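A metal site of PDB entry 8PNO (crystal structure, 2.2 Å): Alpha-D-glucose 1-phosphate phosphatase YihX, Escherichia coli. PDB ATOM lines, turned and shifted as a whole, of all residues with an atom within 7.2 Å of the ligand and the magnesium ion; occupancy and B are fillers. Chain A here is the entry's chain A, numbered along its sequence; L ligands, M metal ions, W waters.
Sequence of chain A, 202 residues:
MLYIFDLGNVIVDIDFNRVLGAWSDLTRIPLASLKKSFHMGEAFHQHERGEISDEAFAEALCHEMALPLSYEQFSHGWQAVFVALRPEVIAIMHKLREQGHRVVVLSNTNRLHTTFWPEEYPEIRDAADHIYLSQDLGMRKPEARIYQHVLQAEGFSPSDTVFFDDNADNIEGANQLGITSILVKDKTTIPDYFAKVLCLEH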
ATOM      1  N   PHE A   5     -29.680  -1.843 -18.054  1.00  0.00           N
ATOM      2  CA  PHE A   5     -29.123  -2.942 -17.280  1.00  0.00           C
ATOM      3  C   PHE A   5     -28.008  -3.640 -18.056  1.00  0.00           C
ATOM      4  O   PHE A   5     -28.190  -3.986 -19.217  1.00  0.00           O
ATOM      5  CB  PHE A   5     -30.205  -3.962 -16.950  1.00  0.00           C
ATOM      6  CG  PHE A   5     -31.288  -3.421 -16.044  1.00  0.00           C
ATOM      7  CD1 PHE A   5     -32.388  -2.746 -16.577  1.00  0.00           C
ATOM      8  CD2 PHE A   5     -31.184  -3.523 -14.672  1.00  0.00           C
ATOM      9  CE1 PHE A   5     -33.375  -2.247 -15.752  1.00  0.00           C
ATOM     10  CE2 PHE A   5     -32.179  -3.029 -13.848  1.00  0.00           C
ATOM     11  CZ  PHE A   5     -33.271  -2.395 -14.385  1.00  0.00           C
ATOM     12  N   ASP A   6     -26.871  -3.810 -17.382  1.00  0.00           N
ATOM     13  CA  ASP A   6     -25.854  -4.806 -17.747  1.00  0.00           C
ATOM     14  C   ASP A   6     -26.487  -6.192 -17.662  1.00  0.00           C
ATOM     15  O   ASP A   6     -27.532  -6.367 -17.040  1.00  0.00           O
ATOM     16  CB  ASP A   6     -24.637  -4.672 -16.815  1.00  0.00           C
ATOM     17  CG  ASP A   6     -23.537  -5.697 -17.041  1.00  0.00           C
ATOM     18  OD1 ASP A   6     -23.274  -5.996 -18.232  1.00  0.00           O
ATOM     19  OD2 ASP A   6     -22.926  -6.139 -16.024  1.00  0.00           O
ATOM     20  N   LEU A   7     -25.868  -7.179 -18.295  1.00  0.00           N
ATOM     21  CA  LEU A   7     -26.453  -8.510 -18.325  1.00  0.00           C
ATOM     22  C   LEU A   7     -25.767  -9.381 -17.291  1.00  0.00           C
ATOM     23  O   LEU A   7     -26.378  -9.783 -16.304  1.00  0.00           O
ATOM     24  CB  LEU A   7     -26.306  -9.039 -19.770  1.00  0.00           C
ATOM     25  CG  LEU A   7     -27.182 -10.219 -20.179  1.00  0.00           C
ATOM     26  CD1 LEU A   7     -28.518 -10.163 -19.469  1.00  0.00           C
ATOM     27  CD2 LEU A   7     -27.397 -10.214 -21.679  1.00  0.00           C
ATOM     28  N   GLY A   8     -24.450  -9.570 -17.453  1.00  0.00           N
ATOM     29  CA  GLY A   8     -23.682 -10.448 -16.598  1.00  0.00           C
ATOM     30  C   GLY A   8     -23.517  -9.899 -15.186  1.00  0.00           C
ATOM     31  O   GLY A   8     -23.033  -8.773 -14.998  1.00  0.00           O
ATOM     32  N   ASN A   9     -23.865 -10.763 -14.225  1.00  0.00           N
ATOM     33  CA  ASN A   9     -23.839 -10.509 -12.787  1.00  0.00           C
ATOM     34  C   ASN A   9     -24.709  -9.293 -12.440  1.00  0.00           C
ATOM     35  O   ASN A   9     -24.454  -8.627 -11.445  1.00  0.00           O
ATOM     36  CB  ASN A   9     -22.410 -10.509 -12.233  1.00  0.00           C
ATOM     37  CG  ASN A   9     -21.817 -11.901 -12.256  1.00  0.00           C
ATOM     38  OD1 ASN A   9     -22.520 -12.892 -12.117  1.00  0.00           O
ATOM     39  ND2 ASN A   9     -20.521 -12.003 -12.494  1.00  0.00           N
ATOM     40  N   VAL A  10     -25.798  -9.135 -13.203  1.00  0.00           N
ATOM     41  CA  VAL A  10     -26.818  -8.127 -12.983  1.00  0.00           C
ATOM     42  C   VAL A  10     -28.190  -8.760 -13.222  1.00  0.00           C
ATOM     43  O   VAL A  10     -29.010  -8.828 -12.311  1.00  0.00           O
ATOM     44  CB  VAL A  10     -26.540  -6.877 -13.840  1.00  0.00           C
ATOM     45  CG1 VAL A  10     -27.728  -5.918 -13.906  1.00  0.00           C
ATOM     46  CG2 VAL A  10     -25.275  -6.164 -13.390  1.00  0.00           C
ATOM     47  N   VAL A  12     -28.372 -11.894 -14.749  1.00  0.00           N
ATOM     48  CA  VAL A  12     -28.081 -13.309 -14.609  1.00  0.00           C
ATOM     49  C   VAL A  12     -26.815 -13.458 -13.771  1.00  0.00           C
ATOM     50  O   VAL A  12     -25.933 -12.618 -13.845  1.00  0.00           O
ATOM     51  CB  VAL A  12     -27.886 -13.985 -15.990  1.00  0.00           C
ATOM     52  CG1 VAL A  12     -29.088 -13.840 -16.902  1.00  0.00           C
ATOM     53  CG2 VAL A  12     -26.634 -13.510 -16.701  1.00  0.00           C
ATOM     54  N   ILE A  14     -23.415 -15.287 -13.975  1.00  0.00           N
ATOM     55  CA  ILE A  14     -22.595 -15.916 -14.998  1.00  0.00           C
ATOM     56  C   ILE A  14     -21.259 -16.321 -14.381  1.00  0.00           C
ATOM     57  O   ILE A  14     -20.733 -15.594 -13.544  1.00  0.00           O
ATOM     58  CB  ILE A  14     -22.465 -14.996 -16.224  1.00  0.00           C
ATOM     59  CG1 ILE A  14     -21.808 -15.714 -17.412  1.00  0.00           C
ATOM     60  CG2 ILE A  14     -21.730 -13.710 -15.882  1.00  0.00           C
ATOM     61  CD1 ILE A  14     -22.364 -15.332 -18.762  1.00  0.00           C
ATOM     62  N   VAL A 105     -31.113  -3.283 -22.259  1.00  0.00           N
ATOM     63  CA  VAL A 105     -29.937  -4.042 -21.870  1.00  0.00           C
ATOM     64  C   VAL A 105     -28.785  -3.501 -22.707  1.00  0.00           C
ATOM     65  O   VAL A 105     -28.965  -3.348 -23.924  1.00  0.00           O
ATOM     66  CB  VAL A 105     -30.132  -5.561 -22.110  1.00  0.00           C
ATOM     67  CG1 VAL A 105     -28.829  -6.320 -21.895  1.00  0.00           C
ATOM     68  CG2 VAL A 105     -31.262  -6.160 -21.277  1.00  0.00           C
ATOM     69  N   LEU A 106     -27.654  -3.251 -22.029  1.00  0.00           N
ATOM     70  CA  LEU A 106     -26.393  -2.942 -22.663  1.00  0.00           C
ATOM     71  C   LEU A 106     -25.344  -3.930 -22.164  1.00  0.00           C
ATOM     72  O   LEU A 106     -25.038  -3.995 -20.971  1.00  0.00           O
ATOM     73  CB  LEU A 106     -25.982  -1.489 -22.374  1.00  0.00           C
ATOM     74  CG  LEU A 106     -24.613  -1.072 -22.921  1.00  0.00           C
ATOM     75  CD1 LEU A 106     -24.537  -1.116 -24.449  1.00  0.00           C
ATOM     76  CD2 LEU A 106     -24.213   0.298 -22.433  1.00  0.00           C
ATOM     77  N   SER A 107     -24.771  -4.680 -23.124  1.00  0.00           N
ATOM     78  CA  SER A 107     -23.927  -5.816 -22.809  1.00  0.00           C
ATOM     79  C   SER A 107     -22.711  -5.882 -23.717  1.00  0.00           C
ATOM     80  O   SER A 107     -22.818  -5.942 -24.951  1.00  0.00           O
ATOM     81  CB  SER A 107     -24.698  -7.082 -22.898  1.00  0.00           C
ATOM     82  OG  SER A 107     -23.919  -8.151 -22.418  1.00  0.00           O
ATOM     83  N   ASN A 108     -21.543  -5.913 -23.058  1.00  0.00           N
ATOM     84  CA  ASN A 108     -20.311  -6.437 -23.640  1.00  0.00           C
ATOM     85  C   ASN A 108     -20.399  -7.969 -23.725  1.00  0.00           C
ATOM     86  O   ASN A 108     -20.510  -8.626 -22.691  1.00  0.00           O
ATOM     87  CB  ASN A 108     -19.111  -6.012 -22.801  1.00  0.00           C
ATOM     88  CG  ASN A 108     -18.715  -4.562 -22.955  1.00  0.00           C
ATOM     89  OD1 ASN A 108     -19.384  -3.810 -23.685  1.00  0.00           O
ATOM     90  ND2 ASN A 108     -17.619  -4.182 -22.318  1.00  0.00           N
ATOM     91  N   THR A 109     -20.348  -8.528 -24.948  1.00  0.00           N
ATOM     92  CA  THR A 109     -20.683  -9.922 -25.191  1.00  0.00           C
ATOM     93  C   THR A 109     -19.623 -10.618 -26.050  1.00  0.00           C
ATOM     94  O   THR A 109     -19.174 -10.090 -27.073  1.00  0.00           O
ATOM     95  CB  THR A 109     -22.076 -10.099 -25.814  1.00  0.00           C
ATOM     96  OG1 THR A 109     -22.376 -11.497 -25.913  1.00  0.00           O
ATOM     97  CG2 THR A 109     -22.174  -9.434 -27.172  1.00  0.00           C
ATOM     98  N   GLU A 119     -28.350 -13.072 -23.864  1.00  0.00           N
ATOM     99  CA  GLU A 119     -29.079 -12.040 -24.596  1.00  0.00           C
ATOM    100  C   GLU A 119     -30.097 -12.686 -25.539  1.00  0.00           C
ATOM    101  O   GLU A 119     -31.005 -11.977 -25.977  1.00  0.00           O
ATOM    102  CB  GLU A 119     -28.185 -11.132 -25.450  1.00  0.00           C
ATOM    103  CG  GLU A 119     -27.215 -11.860 -26.406  1.00  0.00           C
ATOM    104  CD  GLU A 119     -25.843 -12.039 -25.787  1.00  0.00           C
ATOM    105  OE1 GLU A 119     -25.765 -12.266 -24.529  1.00  0.00           O
ATOM    106  OE2 GLU A 119     -24.848 -11.971 -26.553  1.00  0.00           O
ATOM    107  N   TYR A 132     -28.884  -3.808 -26.437  1.00  0.00           N
ATOM    108  CA  TYR A 132     -27.756  -3.226 -27.149  1.00  0.00           C
ATOM    109  C   TYR A 132     -26.555  -4.110 -26.864  1.00  0.00           C
ATOM    110  O   TYR A 132     -26.243  -4.320 -25.706  1.00  0.00           O
ATOM    111  CB  TYR A 132     -27.509  -1.775 -26.689  1.00  0.00           C
ATOM    112  CG  TYR A 132     -28.608  -0.813 -27.050  1.00  0.00           C
ATOM    113  CD1 TYR A 132     -29.694  -0.593 -26.200  1.00  0.00           C
ATOM    114  CD2 TYR A 132     -28.578  -0.122 -28.259  1.00  0.00           C
ATOM    115  CE1 TYR A 132     -30.709   0.281 -26.551  1.00  0.00           C
ATOM    116  CE2 TYR A 132     -29.599   0.747 -28.632  1.00  0.00           C
ATOM    117  CZ  TYR A 132     -30.667   0.958 -27.772  1.00  0.00           C
ATOM    118  OH  TYR A 132     -31.687   1.827 -28.145  1.00  0.00           O
ATOM    119  N   SER A 134     -22.420  -5.176 -27.800  1.00  0.00           N
ATOM    120  CA  SER A 134     -21.149  -4.628 -28.218  1.00  0.00           C
ATOM    121  C   SER A 134     -20.786  -5.107 -29.634  1.00  0.00           C
ATOM    122  O   SER A 134     -20.239  -4.343 -30.413  1.00  0.00           O
ATOM    123  CB  SER A 134     -20.077  -5.016 -27.193  1.00  0.00           C
ATOM    124  OG  SER A 134     -19.924  -6.420 -27.059  1.00  0.00           O
ATOM    125  N   LYS A 141     -18.405  -1.144 -23.583  1.00  0.00           N
ATOM    126  CA  LYS A 141     -18.225  -0.465 -22.304  1.00  0.00           C
ATOM    127  C   LYS A 141     -16.774  -0.682 -21.844  1.00  0.00           C
ATOM    128  O   LYS A 141     -16.223  -1.768 -22.056  1.00  0.00           O
ATOM    129  CB  LYS A 141     -19.225  -0.987 -21.269  1.00  0.00           C
ATOM    130  CG  LYS A 141     -20.705  -0.862 -21.627  1.00  0.00           C
ATOM    131  CD  LYS A 141     -21.636  -1.451 -20.596  1.00  0.00           C
ATOM    132  CE  LYS A 141     -21.438  -2.937 -20.400  1.00  0.00           C
ATOM    133  NZ  LYS A 141     -22.605  -3.562 -19.712  1.00  0.00           N
ATOM    134  N   PHE A 163     -28.246   3.601 -14.781  1.00  0.00           N
ATOM    135  CA  PHE A 163     -27.493   2.481 -15.318  1.00  0.00           C
ATOM    136  C   PHE A 163     -27.032   1.583 -14.188  1.00  0.00           C
ATOM    137  O   PHE A 163     -26.444   2.068 -13.212  1.00  0.00           O
ATOM    138  CB  PHE A 163     -26.301   3.016 -16.124  1.00  0.00           C
ATOM    139  CG  PHE A 163     -25.235   2.038 -16.577  1.00  0.00           C
ATOM    140  CD1 PHE A 163     -25.536   0.971 -17.409  1.00  0.00           C
ATOM    141  CD2 PHE A 163     -23.915   2.221 -16.218  1.00  0.00           C
ATOM    142  CE1 PHE A 163     -24.547   0.099 -17.831  1.00  0.00           C
ATOM    143  CE2 PHE A 163     -22.919   1.356 -16.639  1.00  0.00           C
ATOM    144  CZ  PHE A 163     -23.238   0.287 -17.433  1.00  0.00           C
ATOM    145  N   PHE A 164     -27.278   0.271 -14.341  1.00  0.00           N
ATOM    146  CA  PHE A 164     -26.827  -0.742 -13.392  1.00  0.00           C
ATOM    147  C   PHE A 164     -25.779  -1.653 -14.016  1.00  0.00           C
ATOM    148  O   PHE A 164     -26.058  -2.271 -15.038  1.00  0.00           O
ATOM    149  CB  PHE A 164     -28.015  -1.601 -12.960  1.00  0.00           C
ATOM    150  CG  PHE A 164     -29.092  -0.830 -12.240  1.00  0.00           C
ATOM    151  CD1 PHE A 164     -28.959  -0.518 -10.892  1.00  0.00           C
ATOM    152  CD2 PHE A 164     -30.229  -0.389 -12.910  1.00  0.00           C
ATOM    153  CE1 PHE A 164     -29.952   0.192 -10.228  1.00  0.00           C
ATOM    154  CE2 PHE A 164     -31.217   0.314 -12.241  1.00  0.00           C
ATOM    155  CZ  PHE A 164     -31.074   0.599 -10.902  1.00  0.00           C
ATOM    156  N   ASP A 165     -24.619  -1.771 -13.351  1.00  0.00           N
ATOM    157  CA  ASP A 165     -23.526  -2.640 -13.797  1.00  0.00           C
ATOM    158  C   ASP A 165     -22.640  -3.019 -12.604  1.00  0.00           C
ATOM    159  O   ASP A 165     -22.357  -2.209 -11.719  1.00  0.00           O
ATOM    160  CB  ASP A 165     -22.758  -1.947 -14.915  1.00  0.00           C
ATOM    161  CG  ASP A 165     -21.813  -2.826 -15.734  1.00  0.00           C
ATOM    162  OD1 ASP A 165     -21.049  -3.594 -15.129  1.00  0.00           O
ATOM    163  OD2 ASP A 165     -21.801  -2.647 -16.992  1.00  0.00           O
ATOM    164  N   ASP A 166     -22.150  -4.257 -12.602  1.00  0.00           N
ATOM    165  CA  ASP A 166     -21.340  -4.794 -11.521  1.00  0.00           C
ATOM    166  C   ASP A 166     -19.871  -4.440 -11.667  1.00  0.00           C
ATOM    167  O   ASP A 166     -19.102  -4.709 -10.749  1.00  0.00           O
ATOM    168  CB  ASP A 166     -21.451  -6.324 -11.455  1.00  0.00           C
ATOM    169  CG  ASP A 166     -20.938  -7.068 -12.673  1.00  0.00           C
ATOM    170  OD1 ASP A 166     -21.527  -6.928 -13.765  1.00  0.00           O
ATOM    171  OD2 ASP A 166     -19.944  -7.787 -12.528  1.00  0.00           O
ATOM    172  N   ASN A 167     -19.471  -3.879 -12.816  1.00  0.00           N
ATOM    173  CA  ASN A 167     -18.072  -3.576 -13.089  1.00  0.00           C
ATOM    174  C   ASN A 167     -17.859  -2.079 -12.856  1.00  0.00           C
ATOM    175  O   ASN A 167     -18.639  -1.264 -13.336  1.00  0.00           O
ATOM    176  CB  ASN A 167     -17.683  -4.023 -14.505  1.00  0.00           C
ATOM    177  CG  ASN A 167     -16.287  -3.595 -14.940  1.00  0.00           C
ATOM    178  OD1 ASN A 167     -15.913  -2.421 -14.898  1.00  0.00           O
ATOM    179  ND2 ASN A 167     -15.509  -4.556 -15.375  1.00  0.00           N
ATOM    180  N   ASN A 170     -17.008   0.220 -15.715  1.00  0.00           N
ATOM    181  CA  ASN A 170     -18.190   0.468 -16.518  1.00  0.00           C
ATOM    182  C   ASN A 170     -19.000   1.598 -15.906  1.00  0.00           C
ATOM    183  O   ASN A 170     -19.576   2.422 -16.610  1.00  0.00           O
ATOM    184  CB  ASN A 170     -19.047  -0.792 -16.692  1.00  0.00           C
ATOM    185  CG  ASN A 170     -18.479  -1.728 -17.735  1.00  0.00           C
ATOM    186  OD1 ASN A 170     -17.496  -1.405 -18.404  1.00  0.00           O
ATOM    187  ND2 ASN A 170     -19.081  -2.907 -17.875  1.00  0.00           N
HETATM  188  O1  LIG L   1     -20.648  -6.013 -18.267  1.00  0.00           O
HETATM  189  F1  LIG L   1     -21.667  -8.213 -17.521  1.00  0.00           F
HETATM  190 MG1  LIG L   1     -21.870  -7.116 -18.981  1.00  0.00          MG
HETATM  191  F2  LIG L   1     -21.839  -6.154 -20.496  1.00  0.00           F
HETATM  192  F3  LIG L   1     -23.277  -8.002 -19.637  1.00  0.00           F
HETATM  193 MG    MG M   1     -21.522  -7.569 -15.680  1.00  0.00          MG
HETATM  194  O   HOH W   1     -20.288  -9.066 -15.212  1.00  0.00           O
HETATM  195  O   HOH W   2     -20.703  -8.391 -20.017  1.00  0.00           O
HETATM  196  O   HOH W   3     -20.261  -5.994 -15.883  1.00  0.00           O
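The side-chain amide nitrogen (ND2) of Asn 108 lies within hydrogen-bond range of the backbone carbonyl oxygen (O) of Lys 141 (2.8 Å). NZ of Lys 141 sits at hydrogen-bond distance from O of Leu 106 (2.8 Å). The backbone carbonyl oxygen (O) of Ser 107 is in hydrogen-bond range of the backbone NH (N) of Ser 134. O of Tyr 132 is in hydrogen-bond range of N of Ser 107. The side-chain amide nitrogen of Asn 170 lies within hydrogen-bond range of the side-chain carboxylate of Asp 165 (2.9 Å). The backbone NH (N) of Asn 170 is in hydrogen-bond range of the side-chain amide oxygen (OD1) of Asn 167 (3.0 Å). OD1 of Asp 165 is in hydrogen-bond range of N of Asn 167, at 2.8 Å. The backbone carbonyl oxygen (O) of Phe 5 is in hydrogen-bond range of the backbone NH (N) of Leu 106.
The magnesium ion is bound by F1 of the ligand (2.0 Å), water W1 (2.0 Å), OD1 of Asp 166 (2.0 Å), water W3 (2.0 Å), OD2 of Asp 6 (2.0 Å) and O of Gly 8 (2.0 Å).
OD1 of Asp 6 is bound to MG1 of the ligand. A fluorine (F3) of the ligand is in hydrogen-bond range of the backbone NH (N) of Gly 8 (2.9 Å). The backbone NH of Asn 108 is in hydrogen-bond range of a fluorine (F2) of the ligand, at 2.6 Å. NZ of Lys 141 is in hydrogen-bond range of F2 of the ligand (2.8 Å). OG of Ser 107 is in hydrogen-bond range of F3 of the ligand (2.9 Å). F3 of the ligand is in hydrogen-bond range of N of Leu 7, at 3.0 Å.
Leu 106 touches the ligand (O to F2, 3.9 Å). OD2 of Asp 165 touches O1 of the ligand, at 3.8 Å. Asn 170 touches the ligand. Hydrophobic or aromatic side chains that line the ligand: Leu 7. Ten residues have an atom within 4 Å of the ligand: Asp 6, Leu 7, Gly 8, Leu 106, Ser 107, Asn 108, Lys 141, Asp 165, Asp 166 and Asn 170. The nearest printed residue that does not touch the ligand is Asn 9 (4.7 Å).
Along chain A the residues within 4 Å of the magnesium ion span positions 6 to 166.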
